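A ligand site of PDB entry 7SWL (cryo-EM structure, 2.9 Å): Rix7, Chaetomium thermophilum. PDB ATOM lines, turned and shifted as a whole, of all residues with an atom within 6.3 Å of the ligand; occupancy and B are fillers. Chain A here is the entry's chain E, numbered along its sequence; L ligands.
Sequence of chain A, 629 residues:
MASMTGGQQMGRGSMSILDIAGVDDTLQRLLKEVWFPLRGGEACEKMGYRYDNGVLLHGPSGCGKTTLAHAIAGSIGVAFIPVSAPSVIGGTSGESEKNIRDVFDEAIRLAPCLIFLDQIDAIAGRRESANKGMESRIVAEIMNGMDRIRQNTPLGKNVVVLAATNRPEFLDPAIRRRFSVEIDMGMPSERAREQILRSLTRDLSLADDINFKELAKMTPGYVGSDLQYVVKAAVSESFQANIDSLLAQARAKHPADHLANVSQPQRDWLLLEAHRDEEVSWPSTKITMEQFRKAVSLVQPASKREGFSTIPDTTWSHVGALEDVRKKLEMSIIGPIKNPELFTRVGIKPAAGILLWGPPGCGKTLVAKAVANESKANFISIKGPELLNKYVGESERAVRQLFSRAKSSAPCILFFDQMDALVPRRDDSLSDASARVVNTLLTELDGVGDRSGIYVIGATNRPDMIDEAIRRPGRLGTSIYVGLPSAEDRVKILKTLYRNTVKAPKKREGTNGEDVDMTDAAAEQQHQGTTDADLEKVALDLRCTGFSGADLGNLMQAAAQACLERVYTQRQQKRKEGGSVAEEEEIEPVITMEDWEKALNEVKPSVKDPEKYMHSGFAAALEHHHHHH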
ATOM      1  N   HIS A 318     -21.272  -1.979 -34.345  1.00  0.00           N
ATOM      2  CA  HIS A 318     -22.657  -1.532 -34.465  1.00  0.00           C
ATOM      3  C   HIS A 318     -23.162  -0.830 -33.207  1.00  0.00           C
ATOM      4  O   HIS A 318     -24.239  -0.236 -33.247  1.00  0.00           O
ATOM      5  CB  HIS A 318     -23.573  -2.716 -34.777  1.00  0.00           C
ATOM      6  CG  HIS A 318     -23.314  -3.342 -36.111  1.00  0.00           C
ATOM      7  ND1 HIS A 318     -22.065  -3.670 -36.558  1.00  0.00           N
ATOM      8  CD2 HIS A 318     -24.177  -3.719 -37.088  1.00  0.00           C
ATOM      9  CE1 HIS A 318     -22.145  -4.207 -37.758  1.00  0.00           C
ATOM     10  NE2 HIS A 318     -23.426  -4.257 -38.106  1.00  0.00           N
ATOM     11  N   VAL A 319     -22.424  -0.908 -32.105  1.00  0.00           N
ATOM     12  CA  VAL A 319     -22.833  -0.349 -30.825  1.00  0.00           C
ATOM     13  C   VAL A 319     -22.001   0.898 -30.551  1.00  0.00           C
ATOM     14  O   VAL A 319     -20.765   0.851 -30.627  1.00  0.00           O
ATOM     15  CB  VAL A 319     -22.682  -1.372 -29.688  1.00  0.00           C
ATOM     16  CG1 VAL A 319     -23.232  -0.800 -28.392  1.00  0.00           C
ATOM     17  CG2 VAL A 319     -23.395  -2.666 -30.045  1.00  0.00           C
ATOM     18  N   GLY A 320     -22.667   1.995 -30.225  1.00  0.00           N
ATOM     19  CA  GLY A 320     -21.984   3.235 -29.901  1.00  0.00           C
ATOM     20  C   GLY A 320     -21.760   3.362 -28.404  1.00  0.00           C
ATOM     21  O   GLY A 320     -22.621   3.032 -27.597  1.00  0.00           O
ATOM     22  N   ALA A 321     -20.569   3.857 -28.044  1.00  0.00           N
ATOM     23  CA  ALA A 321     -20.148   3.995 -26.652  1.00  0.00           C
ATOM     24  C   ALA A 321     -20.292   2.681 -25.899  1.00  0.00           C
ATOM     25  O   ALA A 321     -19.939   1.619 -26.426  1.00  0.00           O
ATOM     26  CB  ALA A 321     -20.951   5.095 -25.954  1.00  0.00           C
ATOM     27  N   LEU A 322     -20.808   2.739 -24.673  1.00  0.00           N
ATOM     28  CA  LEU A 322     -21.041   1.566 -23.842  1.00  0.00           C
ATOM     29  C   LEU A 322     -19.753   0.770 -23.637  1.00  0.00           C
ATOM     30  O   LEU A 322     -19.667  -0.422 -23.956  1.00  0.00           O
ATOM     31  CB  LEU A 322     -22.158   0.685 -24.428  1.00  0.00           C
ATOM     32  CG  LEU A 322     -23.522   1.359 -24.536  1.00  0.00           C
ATOM     33  CD1 LEU A 322     -24.534   0.419 -25.167  1.00  0.00           C
ATOM     34  CD2 LEU A 322     -23.994   1.824 -23.170  1.00  0.00           C
ATOM     35  N   PRO A 359     -33.021   2.393 -18.648  1.00  0.00           N
ATOM     36  CA  PRO A 359     -34.197   2.962 -19.294  1.00  0.00           C
ATOM     37  C   PRO A 359     -34.376   2.397 -20.697  1.00  0.00           C
ATOM     38  O   PRO A 359     -33.388   2.032 -21.361  1.00  0.00           O
ATOM     39  CB  PRO A 359     -33.892   4.466 -19.331  1.00  0.00           C
ATOM     40  CG  PRO A 359     -32.417   4.555 -19.221  1.00  0.00           C
ATOM     41  CD  PRO A 359     -31.997   3.405 -18.358  1.00  0.00           C
ATOM     42  N   PRO A 360     -35.609   2.281 -21.169  1.00  0.00           N
ATOM     43  CA  PRO A 360     -35.840   1.716 -22.503  1.00  0.00           C
ATOM     44  C   PRO A 360     -35.254   2.599 -23.593  1.00  0.00           C
ATOM     45  O   PRO A 360     -35.102   3.817 -23.442  1.00  0.00           O
ATOM     46  CB  PRO A 360     -37.360   1.657 -22.614  1.00  0.00           C
ATOM     47  CG  PRO A 360     -37.862   1.745 -21.203  1.00  0.00           C
ATOM     48  CD  PRO A 360     -36.872   2.598 -20.486  1.00  0.00           C
ATOM     49  N   GLY A 361     -34.912   1.956 -24.713  1.00  0.00           N
ATOM     50  CA  GLY A 361     -34.318   2.664 -25.826  1.00  0.00           C
ATOM     51  C   GLY A 361     -32.818   2.853 -25.748  1.00  0.00           C
ATOM     52  O   GLY A 361     -32.271   3.639 -26.532  1.00  0.00           O
ATOM     53  N   CYS A 362     -32.140   2.178 -24.821  1.00  0.00           N
ATOM     54  CA  CYS A 362     -30.700   2.302 -24.661  1.00  0.00           C
ATOM     55  C   CYS A 362     -29.936   1.154 -25.308  1.00  0.00           C
ATOM     56  O   CYS A 362     -28.739   0.982 -25.031  1.00  0.00           O
ATOM     57  CB  CYS A 362     -30.345   2.395 -23.175  1.00  0.00           C
ATOM     58  SG  CYS A 362     -30.888   3.925 -22.393  1.00  0.00           S
ATOM     59  N   GLY A 363     -30.579   0.365 -26.158  1.00  0.00           N
ATOM     60  CA  GLY A 363     -29.893  -0.695 -26.862  1.00  0.00           C
ATOM     61  C   GLY A 363     -29.578  -1.921 -26.034  1.00  0.00           C
ATOM     62  O   GLY A 363     -28.602  -2.607 -26.332  1.00  0.00           O
ATOM     63  N   LYS A 364     -30.379  -2.208 -25.005  1.00  0.00           N
ATOM     64  CA  LYS A 364     -30.135  -3.396 -24.186  1.00  0.00           C
ATOM     65  C   LYS A 364     -30.253  -4.667 -25.018  1.00  0.00           C
ATOM     66  O   LYS A 364     -29.470  -5.606 -24.843  1.00  0.00           O
ATOM     67  CB  LYS A 364     -31.098  -3.427 -23.001  1.00  0.00           C
ATOM     68  CG  LYS A 364     -30.804  -2.367 -21.948  1.00  0.00           C
ATOM     69  CD  LYS A 364     -31.769  -2.474 -20.783  1.00  0.00           C
ATOM     70  CE  LYS A 364     -33.188  -2.216 -21.227  1.00  0.00           C
ATOM     71  NZ  LYS A 364     -34.124  -2.161 -20.070  1.00  0.00           N
ATOM     72  N   THR A 365     -31.241  -4.718 -25.915  1.00  0.00           N
ATOM     73  CA  THR A 365     -31.329  -5.837 -26.844  1.00  0.00           C
ATOM     74  C   THR A 365     -30.126  -5.862 -27.787  1.00  0.00           C
ATOM     75  O   THR A 365     -29.603  -6.933 -28.102  1.00  0.00           O
ATOM     76  CB  THR A 365     -32.624  -5.760 -27.644  1.00  0.00           C
ATOM     77  OG1 THR A 365     -33.739  -5.689 -26.740  1.00  0.00           O
ATOM     78  CG2 THR A 365     -32.782  -6.991 -28.534  1.00  0.00           C
ATOM     79  N   LEU A 366     -29.680  -4.683 -28.229  1.00  0.00           N
ATOM     80  CA  LEU A 366     -28.538  -4.612 -29.129  1.00  0.00           C
ATOM     81  C   LEU A 366     -27.264  -5.108 -28.454  1.00  0.00           C
ATOM     82  O   LEU A 366     -26.438  -5.782 -29.078  1.00  0.00           O
ATOM     83  CB  LEU A 366     -28.359  -3.189 -29.637  1.00  0.00           C
ATOM     84  CG  LEU A 366     -27.427  -2.992 -30.831  1.00  0.00           C
ATOM     85  CD1 LEU A 366     -28.096  -3.443 -32.109  1.00  0.00           C
ATOM     86  CD2 LEU A 366     -26.980  -1.549 -30.937  1.00  0.00           C
ATOM     87  N   VAL A 367     -27.085  -4.770 -27.176  1.00  0.00           N
ATOM     88  CA  VAL A 367     -25.902  -5.200 -26.443  1.00  0.00           C
ATOM     89  C   VAL A 367     -25.862  -6.721 -26.339  1.00  0.00           C
ATOM     90  O   VAL A 367     -24.803  -7.333 -26.532  1.00  0.00           O
ATOM     91  CB  VAL A 367     -25.869  -4.540 -25.045  1.00  0.00           C
ATOM     92  CG1 VAL A 367     -24.746  -5.120 -24.215  1.00  0.00           C
ATOM     93  CG2 VAL A 367     -25.705  -3.041 -25.179  1.00  0.00           C
ATOM     94  N   PHE A 415     -32.428 -14.260 -24.030  1.00  0.00           N
ATOM     95  CA  PHE A 415     -32.652 -12.851 -23.698  1.00  0.00           C
ATOM     96  C   PHE A 415     -34.114 -12.662 -23.326  1.00  0.00           C
ATOM     97  O   PHE A 415     -35.005 -12.992 -24.114  1.00  0.00           O
ATOM     98  CB  PHE A 415     -32.267 -11.959 -24.877  1.00  0.00           C
ATOM     99  CG  PHE A 415     -32.455 -10.498 -24.609  1.00  0.00           C
ATOM    100  CD1 PHE A 415     -31.620  -9.824 -23.745  1.00  0.00           C
ATOM    101  CD2 PHE A 415     -33.464  -9.797 -25.238  1.00  0.00           C
ATOM    102  CE1 PHE A 415     -31.796  -8.478 -23.506  1.00  0.00           C
ATOM    103  CE2 PHE A 415     -33.651  -8.460 -24.998  1.00  0.00           C
ATOM    104  CZ  PHE A 415     -32.809  -7.793 -24.137  1.00  0.00           C
ATOM    105  N   ASP A 417     -36.610  -9.857 -22.540  1.00  0.00           N
ATOM    106  CA  ASP A 417     -36.937  -8.437 -22.536  1.00  0.00           C
ATOM    107  C   ASP A 417     -38.195  -8.203 -21.709  1.00  0.00           C
ATOM    108  O   ASP A 417     -39.143  -8.993 -21.750  1.00  0.00           O
ATOM    109  CB  ASP A 417     -37.136  -7.935 -23.962  1.00  0.00           C
ATOM    110  CG  ASP A 417     -37.112  -6.420 -24.050  1.00  0.00           C
ATOM    111  OD1 ASP A 417     -36.684  -5.774 -23.071  1.00  0.00           O
ATOM    112  OD2 ASP A 417     -37.526  -5.878 -25.089  1.00  0.00           O
ATOM    113  N   PRO A 485     -27.774   7.879 -23.278  1.00  0.00           N
ATOM    114  CA  PRO A 485     -26.892   8.836 -23.977  1.00  0.00           C
ATOM    115  C   PRO A 485     -27.173  10.272 -23.585  1.00  0.00           C
ATOM    116  O   PRO A 485     -28.233  10.815 -23.908  1.00  0.00           O
ATOM    117  CB  PRO A 485     -27.219   8.591 -25.458  1.00  0.00           C
ATOM    118  CG  PRO A 485     -27.787   7.204 -25.501  1.00  0.00           C
ATOM    119  CD  PRO A 485     -28.542   7.045 -24.219  1.00  0.00           C
ATOM    120  N   ASP A 489     -22.457  10.263 -26.064  1.00  0.00           N
ATOM    121  CA  ASP A 489     -22.950   8.985 -26.565  1.00  0.00           C
ATOM    122  C   ASP A 489     -23.852   9.193 -27.780  1.00  0.00           C
ATOM    123  O   ASP A 489     -23.809   8.421 -28.737  1.00  0.00           O
ATOM    124  CB  ASP A 489     -23.687   8.249 -25.442  1.00  0.00           C
ATOM    125  CG  ASP A 489     -24.032   6.818 -25.801  1.00  0.00           C
ATOM    126  OD1 ASP A 489     -23.683   6.364 -26.905  1.00  0.00           O
ATOM    127  OD2 ASP A 489     -24.669   6.140 -24.966  1.00  0.00           O
ATOM    128  N   LYS A 492     -21.700   9.539 -30.872  1.00  0.00           N
ATOM    129  CA  LYS A 492     -21.110   8.282 -31.311  1.00  0.00           C
ATOM    130  C   LYS A 492     -22.144   7.366 -31.949  1.00  0.00           C
ATOM    131  O   LYS A 492     -21.849   6.658 -32.910  1.00  0.00           O
ATOM    132  CB  LYS A 492     -20.435   7.586 -30.124  1.00  0.00           C
ATOM    133  CG  LYS A 492     -19.380   8.437 -29.443  1.00  0.00           C
ATOM    134  CD  LYS A 492     -18.832   7.763 -28.197  1.00  0.00           C
ATOM    135  CE  LYS A 492     -17.806   8.639 -27.499  1.00  0.00           C
ATOM    136  NZ  LYS A 492     -17.281   8.002 -26.264  1.00  0.00           N
ATOM    137  N   ILE A 493     -23.371   7.359 -31.409  1.00  0.00           N
ATOM    138  CA  ILE A 493     -24.417   6.496 -31.955  1.00  0.00           C
ATOM    139  C   ILE A 493     -24.782   6.922 -33.367  1.00  0.00           C
ATOM    140  O   ILE A 493     -24.899   6.080 -34.273  1.00  0.00           O
ATOM    141  CB  ILE A 493     -25.644   6.505 -31.024  1.00  0.00           C
ATOM    142  CG1 ILE A 493     -25.317   5.846 -29.695  1.00  0.00           C
ATOM    143  CG2 ILE A 493     -26.820   5.818 -31.697  1.00  0.00           C
ATOM    144  CD1 ILE A 493     -26.446   5.898 -28.689  1.00  0.00           C
ATOM    145  N   THR A 496     -22.211   5.961 -35.972  1.00  0.00           N
ATOM    146  CA  THR A 496     -22.268   4.526 -36.244  1.00  0.00           C
ATOM    147  C   THR A 496     -23.434   4.182 -37.154  1.00  0.00           C
ATOM    148  O   THR A 496     -23.299   3.369 -38.078  1.00  0.00           O
ATOM    149  CB  THR A 496     -22.357   3.754 -34.929  1.00  0.00           C
ATOM    150  OG1 THR A 496     -21.133   3.909 -34.194  1.00  0.00           O
ATOM    151  CG2 THR A 496     -22.609   2.274 -35.191  1.00  0.00           C
ATOM    152  N   LEU A 497     -24.600   4.781 -36.905  1.00  0.00           N
ATOM    153  CA  LEU A 497     -25.777   4.509 -37.736  1.00  0.00           C
ATOM    154  C   LEU A 497     -25.542   4.949 -39.179  1.00  0.00           C
ATOM    155  O   LEU A 497     -25.914   4.228 -40.116  1.00  0.00           O
ATOM    156  CB  LEU A 497     -26.996   5.204 -37.145  1.00  0.00           C
ATOM    157  CG  LEU A 497     -27.472   4.736 -35.774  1.00  0.00           C
ATOM    158  CD1 LEU A 497     -28.283   5.821 -35.092  1.00  0.00           C
ATOM    159  CD2 LEU A 497     -28.281   3.461 -35.904  1.00  0.00           C
ATOM    160  N   GLY A 549     -31.395   6.605 -26.982  1.00  0.00           N
ATOM    161  CA  GLY A 549     -30.489   5.968 -27.923  1.00  0.00           C
ATOM    162  C   GLY A 549     -31.216   5.372 -29.111  1.00  0.00           C
ATOM    163  O   GLY A 549     -30.709   5.407 -30.239  1.00  0.00           O
ATOM    164  N   ALA A 550     -32.410   4.836 -28.877  1.00  0.00           N
ATOM    165  CA  ALA A 550     -33.216   4.287 -29.961  1.00  0.00           C
ATOM    166  C   ALA A 550     -33.893   5.370 -30.783  1.00  0.00           C
ATOM    167  O   ALA A 550     -34.285   5.105 -31.925  1.00  0.00           O
ATOM    168  CB  ALA A 550     -34.271   3.327 -29.403  1.00  0.00           C
ATOM    169  N   ASP A 551     -34.049   6.573 -30.229  1.00  0.00           N
ATOM    170  CA  ASP A 551     -34.633   7.672 -30.987  1.00  0.00           C
ATOM    171  C   ASP A 551     -33.747   8.056 -32.170  1.00  0.00           C
ATOM    172  O   ASP A 551     -34.239   8.337 -33.266  1.00  0.00           O
ATOM    173  CB  ASP A 551     -34.872   8.878 -30.086  1.00  0.00           C
ATOM    174  CG  ASP A 551     -35.654   8.519 -28.839  1.00  0.00           C
ATOM    175  OD1 ASP A 551     -35.902   7.321 -28.609  1.00  0.00           O
ATOM    176  OD2 ASP A 551     -36.028   9.446 -28.082  1.00  0.00           O
ATOM    177  N   GLY A 553     -31.691   6.149 -33.878  1.00  0.00           N
ATOM    178  CA  GLY A 553     -31.824   5.172 -34.943  1.00  0.00           C
ATOM    179  C   GLY A 553     -33.079   5.373 -35.773  1.00  0.00           C
ATOM    180  O   GLY A 553     -33.038   5.271 -37.005  1.00  0.00           O
ATOM    181  N   ASN A 554     -34.204   5.657 -35.125  1.00  0.00           N
ATOM    182  CA  ASN A 554     -35.427   5.959 -35.857  1.00  0.00           C
ATOM    183  C   ASN A 554     -35.362   7.317 -36.535  1.00  0.00           C
ATOM    184  O   ASN A 554     -35.962   7.509 -37.595  1.00  0.00           O
ATOM    185  CB  ASN A 554     -36.631   5.876 -34.917  1.00  0.00           C
ATOM    186  CG  ASN A 554     -37.943   6.065 -35.650  1.00  0.00           C
ATOM    187  OD1 ASN A 554     -38.443   7.186 -35.786  1.00  0.00           O
ATOM    188  ND2 ASN A 554     -38.525   4.958 -36.119  1.00  0.00           N
HETATM  189  P1  LIG L   1     -34.223  -1.039 -26.655  1.00  0.00           P
HETATM  190  O1  LIG L   1     -33.047  -0.120 -26.871  1.00  0.00           O
HETATM  191  O2  LIG L   1     -35.468  -0.342 -26.176  1.00  0.00           O
HETATM  192  O3  LIG L   1     -33.885  -2.295 -25.880  1.00  0.00           O
HETATM  193  P2  LIG L   1     -33.519  -2.305 -29.063  1.00  0.00           P
HETATM  194  O4  LIG L   1     -32.244  -2.467 -28.260  1.00  0.00           O
HETATM  195  O5  LIG L   1     -34.177  -3.528 -29.653  1.00  0.00           O
HETATM  196  O6  LIG L   1     -34.605  -1.577 -28.122  1.00  0.00           O
HETATM  197  O7  LIG L   1     -33.253  -1.274 -30.268  1.00  0.00           O
HETATM  198  C1  LIG L   1     -32.720   0.028 -30.020  1.00  0.00           C
HETATM  199  C2  LIG L   1     -32.186   0.618 -31.331  1.00  0.00           C
HETATM  200  O8  LIG L   1     -31.472   1.817 -31.049  1.00  0.00           O
HETATM  201  C3  LIG L   1     -31.222  -0.341 -32.009  1.00  0.00           C
HETATM  202  O9  LIG L   1     -31.716  -0.693 -33.305  1.00  0.00           O
HETATM  203  C4  LIG L   1     -29.914   0.406 -32.149  1.00  0.00           C
HETATM  204  O10 LIG L   1     -29.519   0.468 -33.513  1.00  0.00           O
HETATM  205  C5  LIG L   1     -30.158   1.810 -31.609  1.00  0.00           C
HETATM  206  N1  LIG L   1     -29.183   2.084 -30.526  1.00  0.00           N
HETATM  207  C6  LIG L   1     -29.502   2.373 -29.258  1.00  0.00           C
HETATM  208  N2  LIG L   1     -28.391   2.575 -28.506  1.00  0.00           N
HETATM  209  C7  LIG L   1     -27.331   2.410 -29.305  1.00  0.00           C
HETATM  210  C8  LIG L   1     -25.858   2.484 -29.152  1.00  0.00           C
HETATM  211  N3  LIG L   1     -25.289   2.773 -27.962  1.00  0.00           N
HETATM  212  N4  LIG L   1     -25.105   2.244 -30.252  1.00  0.00           N
HETATM  213  C9  LIG L   1     -25.655   1.943 -31.441  1.00  0.00           C
HETATM  214  N5  LIG L   1     -26.979   1.866 -31.653  1.00  0.00           N
HETATM  215  C10 LIG L   1     -27.858   2.084 -30.641  1.00  0.00           C
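O of His 318 touches C9 of the ligand (3.2 Å). Val 319 touches the ligand (C to N4, 3.4 Å). Leu 322 touches the ligand (CD1 to N3, 3.7 Å). Pro 360 touches the ligand (C to O2, 3.9 Å). Lys 364 touches the ligand. CD1 of Ile 493 touches N3 of the ligand, 3.4 Å away. O of Gly 549 touches C6 of the ligand, at 3.4 Å. Ala 550 touches the ligand (CA to O8, 3.2 Å). Hydrophobic or aromatic side chains within 4 Å of the ligand: Leu 322, Leu 366, Ile 493 and Ala 550. Of the 27 residues printed, 14 come within 4 Å of the ligand. The nearest printed residue that does not touch the ligand is Leu 497 (4.03 Å).
The backbone NH (N) of Ala 550 is in hydrogen-bond range of the backbone carbonyl oxygen (O) of Gly 361. The backbone NH (N) of Gly 549 sits at hydrogen-bond distance from the backbone carbonyl oxygen (O) of Gly 361 (3.1 Å). SG of Cys 362 sits at hydrogen-bond distance from O of Pro 359.
N of Gly 320 sits at hydrogen-bond distance from N4 of the ligand, at 2.5 Å. O of Gly 320 is in hydrogen-bond range of N3 of the ligand (2.7 Å). O1 of the ligand sits at hydrogen-bond distance from N of Gly 363 (2.6 Å). O2 of the ligand sits at hydrogen-bond distance from N of Gly 361 (2.8 Å). An oxygen (O1) of the ligand is in hydrogen-bond range of the backbone NH of Cys 362 (3.2 Å). The backbone NH (N) of Thr 365 lies close to an oxygen (O4) of the ligand (3.4 Å). An oxygen (O4) of the ligand lies within hydrogen-bond range of the backbone NH (N) of Leu 366, at 3.4 Å.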
